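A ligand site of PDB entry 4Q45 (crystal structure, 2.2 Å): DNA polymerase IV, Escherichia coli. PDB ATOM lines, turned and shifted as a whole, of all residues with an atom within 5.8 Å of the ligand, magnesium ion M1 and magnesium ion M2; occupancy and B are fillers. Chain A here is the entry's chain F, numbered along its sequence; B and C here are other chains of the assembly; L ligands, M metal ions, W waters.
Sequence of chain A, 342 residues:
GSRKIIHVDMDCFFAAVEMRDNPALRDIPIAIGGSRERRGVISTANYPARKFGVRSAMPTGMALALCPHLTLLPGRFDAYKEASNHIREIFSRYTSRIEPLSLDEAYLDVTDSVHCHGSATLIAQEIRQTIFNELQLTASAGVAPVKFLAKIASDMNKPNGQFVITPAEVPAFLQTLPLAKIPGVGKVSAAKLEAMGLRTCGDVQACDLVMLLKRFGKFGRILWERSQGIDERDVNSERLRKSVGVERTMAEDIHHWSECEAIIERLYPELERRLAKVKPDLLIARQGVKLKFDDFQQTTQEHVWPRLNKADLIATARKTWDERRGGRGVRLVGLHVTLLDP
The backbone NH (N) of Cys 12 is in hydrogen-bond range of an oxygen (O13) of the ligand (3.0 Å).
The side-chain hydroxyl of Ser 43 lies close to an oxygen (O1) of the ligand (3.4 Å).
N1 of the ligand sits at hydrogen-bond distance from N1 of DA 4 of chain B (2.8 Å).
N of Phe 13 lies within hydrogen-bond range of O9 of the ligand.
OG1 of Thr 44 lies within hydrogen-bond range of O9 of the ligand, at 2.9 Å.
The backbone carbonyl oxygen of Ser 43 sits close to a nitrogen (N1) of the ligand (3.4 Å).
The backbone NH of Phe 14 lies within hydrogen-bond range of an oxygen (O3) of the ligand (3.3 Å).
NH1 of Arg 50 lies within salt-bridge range of O12 of the ligand (3.4 Å).
The guanidinium group of Arg 50 sits at hydrogen-bond distance from the backbone carbonyl oxygen of Ala 45, 2.8 Å away.
The backbone carbonyl oxygen of Ser 43 is in hydrogen-bond range of the side-chain hydroxyl of Ser 56 (2.8 Å).
OD2 of Asp 104 sits close to OG of Ser 102 (3.2 Å).
The side-chain hydroxyl of Ser 102 lies close to the backbone NH of Glu 105 (3.4 Å).
O2 of DC 18 of chain C lies close to N2 of DG 5 of chain B (2.5 Å).
The side-chain hydroxyl (OG1) of Thr 44 lies within hydrogen-bond range of the guanidinium group (NH2) of Arg 50 (3.2 Å).
The side-chain hydroxyl (OG) of Ser 102 lies within hydrogen-bond range of O3' of DC 18 of chain C, at 3.0 Å.
The side-chain sulfur (SG) of Cys 12 lies within hydrogen-bond range of the guanidinium group (NH2) of Arg 50 (3.3 Å).
Asp 11 touches the ligand.
CB of Ser 56 touches C4 of the ligand, at 3.8 Å.
CE of Lys 158 touches O12 of the ligand, at 3.1 Å.
DG 5 of chain B touches the ligand.
Hydrophobic or aromatic side chains that line the ligand: Phe 13 and Phe 14.
16 residues have an atom within 4 Å of the ligand: Asp 9, Met 10, Asp 11, Cys 12, Phe 13, Phe 14, Ser 43, Thr 44, Arg 50, Ser 56, Asp 104, Glu 105, Lys 158, DA 4 of chain B, DG 5 of chain B and DC 18 of chain C.
Of the 23 residues printed, 3 come within 4 Å of magnesium ion M1.
Along chain A the residues within 4 Å of magnesium ion M1 span positions 9 to 104.
Within 4 Å of magnesium ion M2: Asp 9, Asp 104, Glu 105 and DC 18 of chain C.
The nearest printed residue that does not touch magnesium ion M2 is Ser 102 (4.04 Å).
Magnesium ion M1 is bound by the side-chain carboxylate of Asp 9, an oxygen (O7) of the ligand, an oxygen (O8) of the ligand, an oxygen (O11) of the ligand, the backbone carbonyl oxygen of Met 10 and the side-chain carboxylate of Asp 104.
Magnesium ion M2 is bound by the side-chain carboxylate (OD2) of Asp 104 (2.1 Å) and the side-chain carboxylate (OE1) of Glu 105 (2.2 Å).
Slightly farther from magnesium ion M2 lies O7 of the ligand (2.6 Å).
Slightly farther from magnesium ion M2 lies OD1 of Asp 104 (2.8 Å).
Slightly farther from magnesium ion M2 lies O3' of DC 18 of chain C (2.8 Å).
Water W3 lies within hydrogen-bond range of the side-chain hydroxyl (OH) of Tyr 47 (2.4 Å), an oxygen (O13) of the ligand (2.5 Å) and the side-chain carboxylate (OD1) of Asp 11 (3.1 Å).
Water W1 lies within hydrogen-bond range of OG of Ser 56 and N3 of the ligand.
Water W2 lies within hydrogen-bond range of the side-chain hydroxyl (OG) of Ser 43 and an oxygen (O1) of the ligand.
Water W7 lies within hydrogen-bond range of OD1 of Asp 11, O of Asp 9 and O13 of the ligand.
Water W6 bridges OP2 of DC 18 of chain C (2.4 Å) and an oxygen (O6) of the ligand (3.3 Å).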
ATOM      1  N   ASP A   9       0.305 -15.798 -21.085  1.00  0.00           N
ATOM      2  CA  ASP A   9       0.101 -17.063 -21.772  1.00  0.00           C
ATOM      3  C   ASP A   9       1.460 -17.730 -21.988  1.00  0.00           C
ATOM      4  O   ASP A   9       2.310 -17.191 -22.690  1.00  0.00           O
ATOM      5  CB  ASP A   9      -0.582 -16.803 -23.122  1.00  0.00           C
ATOM      6  CG  ASP A   9      -1.057 -18.075 -23.818  1.00  0.00           C
ATOM      7  OD1 ASP A   9      -0.393 -19.128 -23.710  1.00  0.00           O
ATOM      8  OD2 ASP A   9      -2.112 -18.012 -24.486  1.00  0.00           O
ATOM      9  N   MET A  10       1.659 -18.902 -21.393  1.00  0.00           N
ATOM     10  CA  MET A  10       2.920 -19.634 -21.530  1.00  0.00           C
ATOM     11  C   MET A  10       3.117 -20.153 -22.957  1.00  0.00           C
ATOM     12  O   MET A  10       2.145 -20.536 -23.619  1.00  0.00           O
ATOM     13  CB  MET A  10       2.964 -20.808 -20.548  1.00  0.00           C
ATOM     14  CG  MET A  10       2.692 -20.430 -19.090  1.00  0.00           C
ATOM     15  SD  MET A  10       3.997 -19.425 -18.358  1.00  0.00           S
ATOM     16  CE  MET A  10       5.333 -20.597 -18.369  1.00  0.00           C
ATOM     17  N   ASP A  11       4.363 -20.163 -23.427  1.00  0.00           N
ATOM     18  CA  ASP A  11       4.679 -20.632 -24.776  1.00  0.00           C
ATOM     19  C   ASP A  11       4.762 -22.152 -24.836  1.00  0.00           C
ATOM     20  O   ASP A  11       5.402 -22.763 -23.985  1.00  0.00           O
ATOM     21  CB  ASP A  11       6.026 -20.065 -25.233  1.00  0.00           C
ATOM     22  CG  ASP A  11       6.069 -18.557 -25.249  1.00  0.00           C
ATOM     23  OD1 ASP A  11       5.086 -17.921 -25.672  1.00  0.00           O
ATOM     24  OD2 ASP A  11       7.113 -17.993 -24.825  1.00  0.00           O
ATOM     25  N   CYS A  12       4.136 -22.752 -25.843  1.00  0.00           N
ATOM     26  CA  CYS A  12       4.199 -24.203 -26.097  1.00  0.00           C
ATOM     27  C   CYS A  12       4.139 -25.022 -24.800  1.00  0.00           C
ATOM     28  O   CYS A  12       4.926 -25.939 -24.604  1.00  0.00           O
ATOM     29  CB  CYS A  12       5.476 -24.558 -26.868  1.00  0.00           C
ATOM     30  SG  CYS A  12       5.494 -23.916 -28.549  1.00  0.00           S
ATOM     31  N   PHE A  13       3.167 -24.683 -23.948  1.00  0.00           N
ATOM     32  CA  PHE A  13       3.212 -25.001 -22.516  1.00  0.00           C
ATOM     33  C   PHE A  13       3.705 -26.398 -22.139  1.00  0.00           C
ATOM     34  O   PHE A  13       4.806 -26.537 -21.566  1.00  0.00           O
ATOM     35  CB  PHE A  13       1.862 -24.716 -21.871  1.00  0.00           C
ATOM     36  CG  PHE A  13       1.888 -24.818 -20.375  1.00  0.00           C
ATOM     37  CD1 PHE A  13       2.891 -24.209 -19.649  1.00  0.00           C
ATOM     38  CD2 PHE A  13       0.905 -25.530 -19.698  1.00  0.00           C
ATOM     39  CE1 PHE A  13       2.922 -24.305 -18.266  1.00  0.00           C
ATOM     40  CE2 PHE A  13       0.930 -25.624 -18.309  1.00  0.00           C
ATOM     41  CZ  PHE A  13       1.943 -25.008 -17.603  1.00  0.00           C
ATOM     42  N   PHE A  14       2.912 -27.420 -22.448  1.00  0.00           N
ATOM     43  CA  PHE A  14       3.263 -28.790 -22.086  1.00  0.00           C
ATOM     44  C   PHE A  14       4.643 -29.129 -22.666  1.00  0.00           C
ATOM     45  O   PHE A  14       5.538 -29.612 -21.958  1.00  0.00           O
ATOM     46  CB  PHE A  14       2.227 -29.803 -22.603  1.00  0.00           C
ATOM     47  CG  PHE A  14       0.861 -29.686 -21.961  1.00  0.00           C
ATOM     48  CD1 PHE A  14       0.579 -28.711 -21.022  1.00  0.00           C
ATOM     49  CD2 PHE A  14      -0.142 -30.589 -22.304  1.00  0.00           C
ATOM     50  CE1 PHE A  14      -0.680 -28.617 -20.442  1.00  0.00           C
ATOM     51  CE2 PHE A  14      -1.405 -30.505 -21.723  1.00  0.00           C
ATOM     52  CZ  PHE A  14      -1.672 -29.514 -20.792  1.00  0.00           C
ATOM     53  N   ALA A  15       4.808 -28.851 -23.953  1.00  0.00           N
ATOM     54  CA  ALA A  15       6.070 -29.111 -24.635  1.00  0.00           C
ATOM     55  C   ALA A  15       7.231 -28.363 -23.989  1.00  0.00           C
ATOM     56  O   ALA A  15       8.311 -28.926 -23.822  1.00  0.00           O
ATOM     57  CB  ALA A  15       5.967 -28.749 -26.111  1.00  0.00           C
ATOM     58  N   ILE A  42      -3.164 -34.529 -30.979  1.00  0.00           N
ATOM     59  CA  ILE A  42      -2.108 -33.708 -30.421  1.00  0.00           C
ATOM     60  C   ILE A  42      -2.652 -32.698 -29.401  1.00  0.00           C
ATOM     61  O   ILE A  42      -3.500 -31.878 -29.730  1.00  0.00           O
ATOM     62  CB  ILE A  42      -1.382 -32.955 -31.562  1.00  0.00           C
ATOM     63  CG1 ILE A  42      -0.857 -33.958 -32.589  1.00  0.00           C
ATOM     64  CG2 ILE A  42      -0.256 -32.077 -31.019  1.00  0.00           C
ATOM     65  CD1 ILE A  42       0.037 -35.039 -31.991  1.00  0.00           C
ATOM     66  N   SER A  43      -2.162 -32.782 -28.164  1.00  0.00           N
ATOM     67  CA  SER A  43      -2.452 -31.770 -27.163  1.00  0.00           C
ATOM     68  C   SER A  43      -1.667 -30.524 -27.532  1.00  0.00           C
ATOM     69  O   SER A  43      -2.229 -29.426 -27.619  1.00  0.00           O
ATOM     70  CB  SER A  43      -2.060 -32.232 -25.759  1.00  0.00           C
ATOM     71  OG  SER A  43      -3.014 -33.122 -25.225  1.00  0.00           O
ATOM     72  N   THR A  44      -0.362 -30.693 -27.778  1.00  0.00           N
ATOM     73  CA  THR A  44       0.430 -29.585 -28.341  1.00  0.00           C
ATOM     74  C   THR A  44       1.764 -30.034 -28.918  1.00  0.00           C
ATOM     75  O   THR A  44       2.156 -31.190 -28.796  1.00  0.00           O
ATOM     76  CB  THR A  44       0.669 -28.423 -27.333  1.00  0.00           C
ATOM     77  OG1 THR A  44       1.049 -27.246 -28.044  1.00  0.00           O
ATOM     78  CG2 THR A  44       1.758 -28.774 -26.337  1.00  0.00           C
ATOM     79  N   ALA A  45       2.465 -29.096 -29.555  1.00  0.00           N
ATOM     80  CA  ALA A  45       3.733 -29.411 -30.207  1.00  0.00           C
ATOM     81  C   ALA A  45       4.737 -28.274 -30.019  1.00  0.00           C
ATOM     82  O   ALA A  45       4.356 -27.116 -29.873  1.00  0.00           O
ATOM     83  CB  ALA A  45       3.516 -29.695 -31.679  1.00  0.00           C
ATOM     84  N   TYR A  47       8.062 -25.899 -31.404  1.00  0.00           N
ATOM     85  CA  TYR A  47       8.281 -25.211 -32.682  1.00  0.00           C
ATOM     86  C   TYR A  47       8.888 -26.076 -33.805  1.00  0.00           C
ATOM     87  O   TYR A  47       8.447 -25.978 -34.957  1.00  0.00           O
ATOM     88  CB  TYR A  47       9.034 -23.883 -32.467  1.00  0.00           C
ATOM     89  CG  TYR A  47       8.139 -22.783 -31.934  1.00  0.00           C
ATOM     90  CD1 TYR A  47       8.084 -22.497 -30.577  1.00  0.00           C
ATOM     91  CD2 TYR A  47       7.339 -22.040 -32.790  1.00  0.00           C
ATOM     92  CE1 TYR A  47       7.250 -21.511 -30.097  1.00  0.00           C
ATOM     93  CE2 TYR A  47       6.512 -21.056 -32.317  1.00  0.00           C
ATOM     94  CZ  TYR A  47       6.473 -20.788 -30.967  1.00  0.00           C
ATOM     95  OH  TYR A  47       5.639 -19.802 -30.501  1.00  0.00           O
ATOM     96  N   ARG A  50       5.857 -27.819 -35.088  1.00  0.00           N
ATOM     97  CA  ARG A  50       4.928 -26.898 -35.739  1.00  0.00           C
ATOM     98  C   ARG A  50       5.421 -26.499 -37.126  1.00  0.00           C
ATOM     99  O   ARG A  50       4.616 -26.232 -38.018  1.00  0.00           O
ATOM    100  CB  ARG A  50       4.715 -25.651 -34.879  1.00  0.00           C
ATOM    101  CG  ARG A  50       4.052 -25.947 -33.539  1.00  0.00           C
ATOM    102  CD  ARG A  50       3.783 -24.688 -32.722  1.00  0.00           C
ATOM    103  NE  ARG A  50       3.263 -25.045 -31.407  1.00  0.00           N
ATOM    104  CZ  ARG A  50       2.830 -24.160 -30.503  1.00  0.00           C
ATOM    105  NH1 ARG A  50       2.845 -22.863 -30.760  1.00  0.00           N
ATOM    106  NH2 ARG A  50       2.382 -24.594 -29.334  1.00  0.00           N
ATOM    107  N   SER A  56      -2.124 -28.304 -32.377  1.00  0.00           N
ATOM    108  CA  SER A  56      -3.034 -28.821 -31.351  1.00  0.00           C
ATOM    109  C   SER A  56      -4.342 -29.258 -31.993  1.00  0.00           C
ATOM    110  O   SER A  56      -4.749 -28.682 -32.997  1.00  0.00           O
ATOM    111  CB  SER A  56      -3.318 -27.755 -30.295  1.00  0.00           C
ATOM    112  OG  SER A  56      -2.157 -27.427 -29.559  1.00  0.00           O
ATOM    113  N   ALA A  57      -4.970 -30.282 -31.423  1.00  0.00           N
ATOM    114  CA  ALA A  57      -6.239 -30.819 -31.900  1.00  0.00           C
ATOM    115  C   ALA A  57      -6.146 -31.584 -33.220  1.00  0.00           C
ATOM    116  O   ALA A  57      -7.152 -32.079 -33.724  1.00  0.00           O
ATOM    117  CB  ALA A  57      -7.328 -29.719 -31.984  1.00  0.00           C
ATOM    118  N   SER A 102      -7.086 -21.257 -17.437  1.00  0.00           N
ATOM    119  CA  SER A 102      -6.541 -22.563 -17.741  1.00  0.00           C
ATOM    120  C   SER A 102      -5.232 -22.654 -16.977  1.00  0.00           C
ATOM    121  O   SER A 102      -4.841 -21.695 -16.316  1.00  0.00           O
ATOM    122  CB  SER A 102      -6.253 -22.700 -19.241  1.00  0.00           C
ATOM    123  OG  SER A 102      -5.312 -21.726 -19.665  1.00  0.00           O
ATOM    124  N   ASP A 104      -2.172 -22.511 -18.052  1.00  0.00           N
ATOM    125  CA  ASP A 104      -1.085 -21.686 -18.562  1.00  0.00           C
ATOM    126  C   ASP A 104      -1.465 -20.237 -18.898  1.00  0.00           C
ATOM    127  O   ASP A 104      -0.646 -19.487 -19.429  1.00  0.00           O
ATOM    128  CB  ASP A 104      -0.487 -22.356 -19.803  1.00  0.00           C
ATOM    129  CG  ASP A 104      -1.191 -21.957 -21.087  1.00  0.00           C
ATOM    130  OD1 ASP A 104      -0.504 -21.737 -22.114  1.00  0.00           O
ATOM    131  OD2 ASP A 104      -2.444 -21.859 -21.094  1.00  0.00           O
ATOM    132  N   GLU A 105      -2.703 -19.847 -18.608  1.00  0.00           N
ATOM    133  CA  GLU A 105      -3.179 -18.522 -18.998  1.00  0.00           C
ATOM    134  C   GLU A 105      -3.806 -17.777 -17.830  1.00  0.00           C
ATOM    135  O   GLU A 105      -4.346 -18.406 -16.910  1.00  0.00           O
ATOM    136  CB  GLU A 105      -4.228 -18.614 -20.115  1.00  0.00           C
ATOM    137  CG  GLU A 105      -3.674 -19.008 -21.471  1.00  0.00           C
ATOM    138  CD  GLU A 105      -4.746 -18.970 -22.550  1.00  0.00           C
ATOM    139  OE1 GLU A 105      -4.514 -19.517 -23.642  1.00  0.00           O
ATOM    140  OE2 GLU A 105      -5.812 -18.370 -22.286  1.00  0.00           O
ATOM    141  N   ASP A 155      -1.057 -13.141 -28.172  1.00  0.00           N
ATOM    142  CA  ASP A 155      -0.774 -14.045 -29.282  1.00  0.00           C
ATOM    143  C   ASP A 155       0.031 -13.379 -30.398  1.00  0.00           C
ATOM    144  O   ASP A 155       0.588 -14.055 -31.272  1.00  0.00           O
ATOM    145  CB  ASP A 155      -2.090 -14.554 -29.886  1.00  0.00           C
ATOM    146  CG  ASP A 155      -2.504 -15.895 -29.341  1.00  0.00           C
ATOM    147  OD1 ASP A 155      -1.606 -16.726 -29.047  1.00  0.00           O
ATOM    148  OD2 ASP A 155      -3.716 -16.137 -29.224  1.00  0.00           O
ATOM    149  N   LYS A 158       4.393 -13.854 -29.844  1.00  0.00           N
ATOM    150  CA  LYS A 158       4.964 -15.049 -29.231  1.00  0.00           C
ATOM    151  C   LYS A 158       5.895 -15.753 -30.214  1.00  0.00           C
ATOM    152  O   LYS A 158       5.737 -15.622 -31.429  1.00  0.00           O
ATOM    153  CB  LYS A 158       3.851 -15.993 -28.739  1.00  0.00           C
ATOM    154  CG  LYS A 158       3.043 -16.651 -29.851  1.00  0.00           C
ATOM    155  CD  LYS A 158       1.977 -17.569 -29.268  1.00  0.00           C
ATOM    156  CE  LYS A 158       1.176 -18.261 -30.372  1.00  0.00           C
ATOM    157  NZ  LYS A 158       0.282 -17.336 -31.136  1.00  0.00           N
ATOM    158  P    DA B   4     -11.425 -37.498 -30.836  1.00  0.00           P
ATOM    159  OP1  DA B   4     -12.030 -38.853 -30.957  1.00  0.00           O
ATOM    160  OP2  DA B   4     -12.308 -36.317 -30.729  1.00  0.00           O
ATOM    161  O5'  DA B   4     -10.449 -37.481 -29.569  1.00  0.00           O
ATOM    162  C5'  DA B   4      -9.395 -38.424 -29.468  1.00  0.00           C
ATOM    163  C4'  DA B   4      -8.807 -38.394 -28.070  1.00  0.00           C
ATOM    164  O4'  DA B   4      -8.075 -37.155 -27.881  1.00  0.00           O
ATOM    165  C3'  DA B   4      -9.842 -38.434 -26.960  1.00  0.00           C
ATOM    166  O3'  DA B   4      -9.313 -39.134 -25.860  1.00  0.00           O
ATOM    167  C2'  DA B   4     -10.064 -36.957 -26.595  1.00  0.00           C
ATOM    168  C1'  DA B   4      -8.709 -36.326 -26.913  1.00  0.00           C
ATOM    169  N9   DA B   4      -8.798 -34.982 -27.477  1.00  0.00           N
ATOM    170  C8   DA B   4      -9.693 -34.527 -28.418  1.00  0.00           C
ATOM    171  N7   DA B   4      -9.522 -33.263 -28.729  1.00  0.00           N
ATOM    172  C5   DA B   4      -8.467 -32.857 -27.940  1.00  0.00           C
ATOM    173  C6   DA B   4      -7.812 -31.620 -27.808  1.00  0.00           C
ATOM    174  N6   DA B   4      -8.147 -30.524 -28.501  1.00  0.00           N
ATOM    175  N1   DA B   4      -6.786 -31.557 -26.931  1.00  0.00           N
ATOM    176  C2   DA B   4      -6.451 -32.653 -26.238  1.00  0.00           C
ATOM    177  N3   DA B   4      -6.992 -33.870 -26.284  1.00  0.00           N
ATOM    178  C4   DA B   4      -8.013 -33.902 -27.155  1.00  0.00           C
ATOM    179  P    DG B   5     -10.283 -39.567 -24.653  1.00  0.00           P
ATOM    180  OP1  DG B   5      -9.754 -40.834 -24.109  1.00  0.00           O
ATOM    181  OP2  DG B   5     -11.684 -39.463 -25.121  1.00  0.00           O
ATOM    182  O5'  DG B   5     -10.069 -38.425 -23.560  1.00  0.00           O
ATOM    183  C5'  DG B   5      -8.782 -38.155 -23.026  1.00  0.00           C
ATOM    184  C4'  DG B   5      -8.915 -36.919 -22.172  1.00  0.00           C
ATOM    185  O4'  DG B   5      -8.961 -35.742 -23.028  1.00  0.00           O
ATOM    186  C3'  DG B   5     -10.194 -36.898 -21.335  1.00  0.00           C
ATOM    187  O3'  DG B   5      -9.829 -36.485 -20.021  1.00  0.00           O
ATOM    188  C2'  DG B   5     -11.071 -35.892 -22.072  1.00  0.00           C
ATOM    189  C1'  DG B   5     -10.030 -34.919 -22.601  1.00  0.00           C
ATOM    190  N9   DG B   5     -10.436 -34.053 -23.712  1.00  0.00           N
ATOM    191  C8   DG B   5     -11.384 -34.302 -24.682  1.00  0.00           C
ATOM    192  N7   DG B   5     -11.510 -33.319 -25.533  1.00  0.00           N
ATOM    193  C5   DG B   5     -10.596 -32.367 -25.122  1.00  0.00           C
ATOM    194  C6   DG B   5     -10.290 -31.100 -25.665  1.00  0.00           C
ATOM    195  O6   DG B   5     -10.774 -30.546 -26.662  1.00  0.00           O
ATOM    196  N1   DG B   5      -9.294 -30.455 -24.947  1.00  0.00           N
ATOM    197  C2   DG B   5      -8.686 -30.981 -23.830  1.00  0.00           C
ATOM    198  N2   DG B   5      -7.751 -30.228 -23.243  1.00  0.00           N
ATOM    199  N3   DG B   5      -8.968 -32.172 -23.309  1.00  0.00           N
ATOM    200  C4   DG B   5      -9.923 -32.812 -24.006  1.00  0.00           C
ATOM    201  P    DC C  18      -8.184 -19.948 -25.076  1.00  0.00           P
ATOM    202  OP1  DC C  18      -7.955 -18.849 -24.123  1.00  0.00           O
ATOM    203  OP2  DC C  18      -7.743 -19.843 -26.490  1.00  0.00           O
ATOM    204  O5'  DC C  18      -7.563 -21.284 -24.459  1.00  0.00           O
ATOM    205  C5'  DC C  18      -7.786 -21.568 -23.094  1.00  0.00           C
ATOM    206  C4'  DC C  18      -7.162 -22.889 -22.724  1.00  0.00           C
ATOM    207  O4'  DC C  18      -7.976 -23.972 -23.230  1.00  0.00           O
ATOM    208  C3'  DC C  18      -5.763 -23.105 -23.293  1.00  0.00           C
ATOM    209  O3'  DC C  18      -4.813 -23.126 -22.237  1.00  0.00           O
ATOM    210  C2'  DC C  18      -5.834 -24.459 -24.004  1.00  0.00           C
ATOM    211  C1'  DC C  18      -7.153 -25.070 -23.559  1.00  0.00           C
ATOM    212  N1   DC C  18      -7.835 -25.864 -24.609  1.00  0.00           N
ATOM    213  C2   DC C  18      -8.017 -27.235 -24.436  1.00  0.00           C
ATOM    214  O2   DC C  18      -7.598 -27.761 -23.399  1.00  0.00           O
ATOM    215  N3   DC C  18      -8.642 -27.943 -25.411  1.00  0.00           N
ATOM    216  C4   DC C  18      -9.086 -27.332 -26.508  1.00  0.00           C
ATOM    217  N4   DC C  18      -9.703 -28.075 -27.433  1.00  0.00           N
ATOM    218  C5   DC C  18      -8.910 -25.938 -26.711  1.00  0.00           C
ATOM    219  C6   DC C  18      -8.282 -25.242 -25.742  1.00  0.00           C
HETATM  220  O1  LIG L   1      -4.343 -30.078 -24.725  1.00  0.00           O
HETATM  221  O2  LIG L   1      -6.528 -28.212 -28.265  1.00  0.00           O
HETATM  222  C1  LIG L   1      -5.625 -28.104 -27.206  1.00  0.00           C
HETATM  223  C2  LIG L   1      -4.982 -26.891 -26.946  1.00  0.00           C
HETATM  224  C3  LIG L   1      -4.092 -26.833 -25.879  1.00  0.00           C
HETATM  225  C4  LIG L   1      -5.232 -25.673 -27.826  1.00  0.00           C
HETATM  226  N1  LIG L   1      -5.386 -29.169 -26.416  1.00  0.00           N
HETATM  227  C5  LIG L   1      -4.520 -29.079 -25.399  1.00  0.00           C
HETATM  228  N2  LIG L   1      -3.878 -27.942 -25.123  1.00  0.00           N
HETATM  229  C6  LIG L   1      -2.939 -27.837 -24.000  1.00  0.00           C
HETATM  230  C7  LIG L   1      -1.543 -27.908 -24.460  1.00  0.00           C
HETATM  231  C8  LIG L   1      -1.102 -26.509 -24.441  1.00  0.00           C
HETATM  232  O3  LIG L   1       0.277 -26.458 -24.190  1.00  0.00           O
HETATM  233  O4  LIG L   1      -3.073 -26.625 -23.252  1.00  0.00           O
HETATM  234  C9  LIG L   1      -1.830 -25.940 -23.339  1.00  0.00           C
HETATM  235  C10 LIG L   1      -2.016 -24.461 -23.561  1.00  0.00           C
HETATM  236  O5  LIG L   1      -2.815 -24.060 -24.647  1.00  0.00           O
HETATM  237  P1  LIG L   1      -2.342 -23.028 -25.728  1.00  0.00           P
HETATM  238  O6  LIG L   1      -3.578 -22.686 -26.484  1.00  0.00           O
HETATM  239  O7  LIG L   1      -1.753 -21.739 -25.074  1.00  0.00           O
HETATM  240  N3  LIG L   1      -1.230 -23.722 -26.787  1.00  0.00           N
HETATM  241  P2  LIG L   1       0.333 -23.623 -26.338  1.00  0.00           P
HETATM  242  O8  LIG L   1       0.466 -22.887 -25.050  1.00  0.00           O
HETATM  243  O9  LIG L   1       0.889 -25.063 -26.185  1.00  0.00           O
HETATM  244  O10 LIG L   1       1.187 -22.913 -27.484  1.00  0.00           O
HETATM  245  P3  LIG L   1       1.243 -21.327 -27.650  1.00  0.00           P
HETATM  246  O11 LIG L   1       0.475 -20.665 -26.509  1.00  0.00           O
HETATM  247  O12 LIG L   1       0.632 -20.946 -28.982  1.00  0.00           O
HETATM  248  O13 LIG L   1       2.671 -20.890 -27.629  1.00  0.00           O
HETATM  249 MG    MG M   1      -0.028 -20.973 -24.275  1.00  0.00          MG
HETATM  250 MG    MG M   2      -3.084 -21.003 -22.957  1.00  0.00          MG
HETATM  251  O   HOH W   1      -1.882 -24.823 -29.152  1.00  0.00           O
HETATM  252  O   HOH W   2      -4.005 -32.398 -23.154  1.00  0.00           O
HETATM  253  O   HOH W   3       4.606 -19.545 -28.317  1.00  0.00           O
HETATM  254  O   HOH W   4      -7.411 -26.647 -30.080  1.00  0.00           O
HETATM  255  O   HOH W   5      -3.859 -21.894 -28.844  1.00  0.00           O
HETATM  256  O   HOH W   6      -6.796 -21.983 -27.070  1.00  0.00           O
HETATM  257  O   HOH W   7       1.984 -18.077 -25.772  1.00  0.00           O
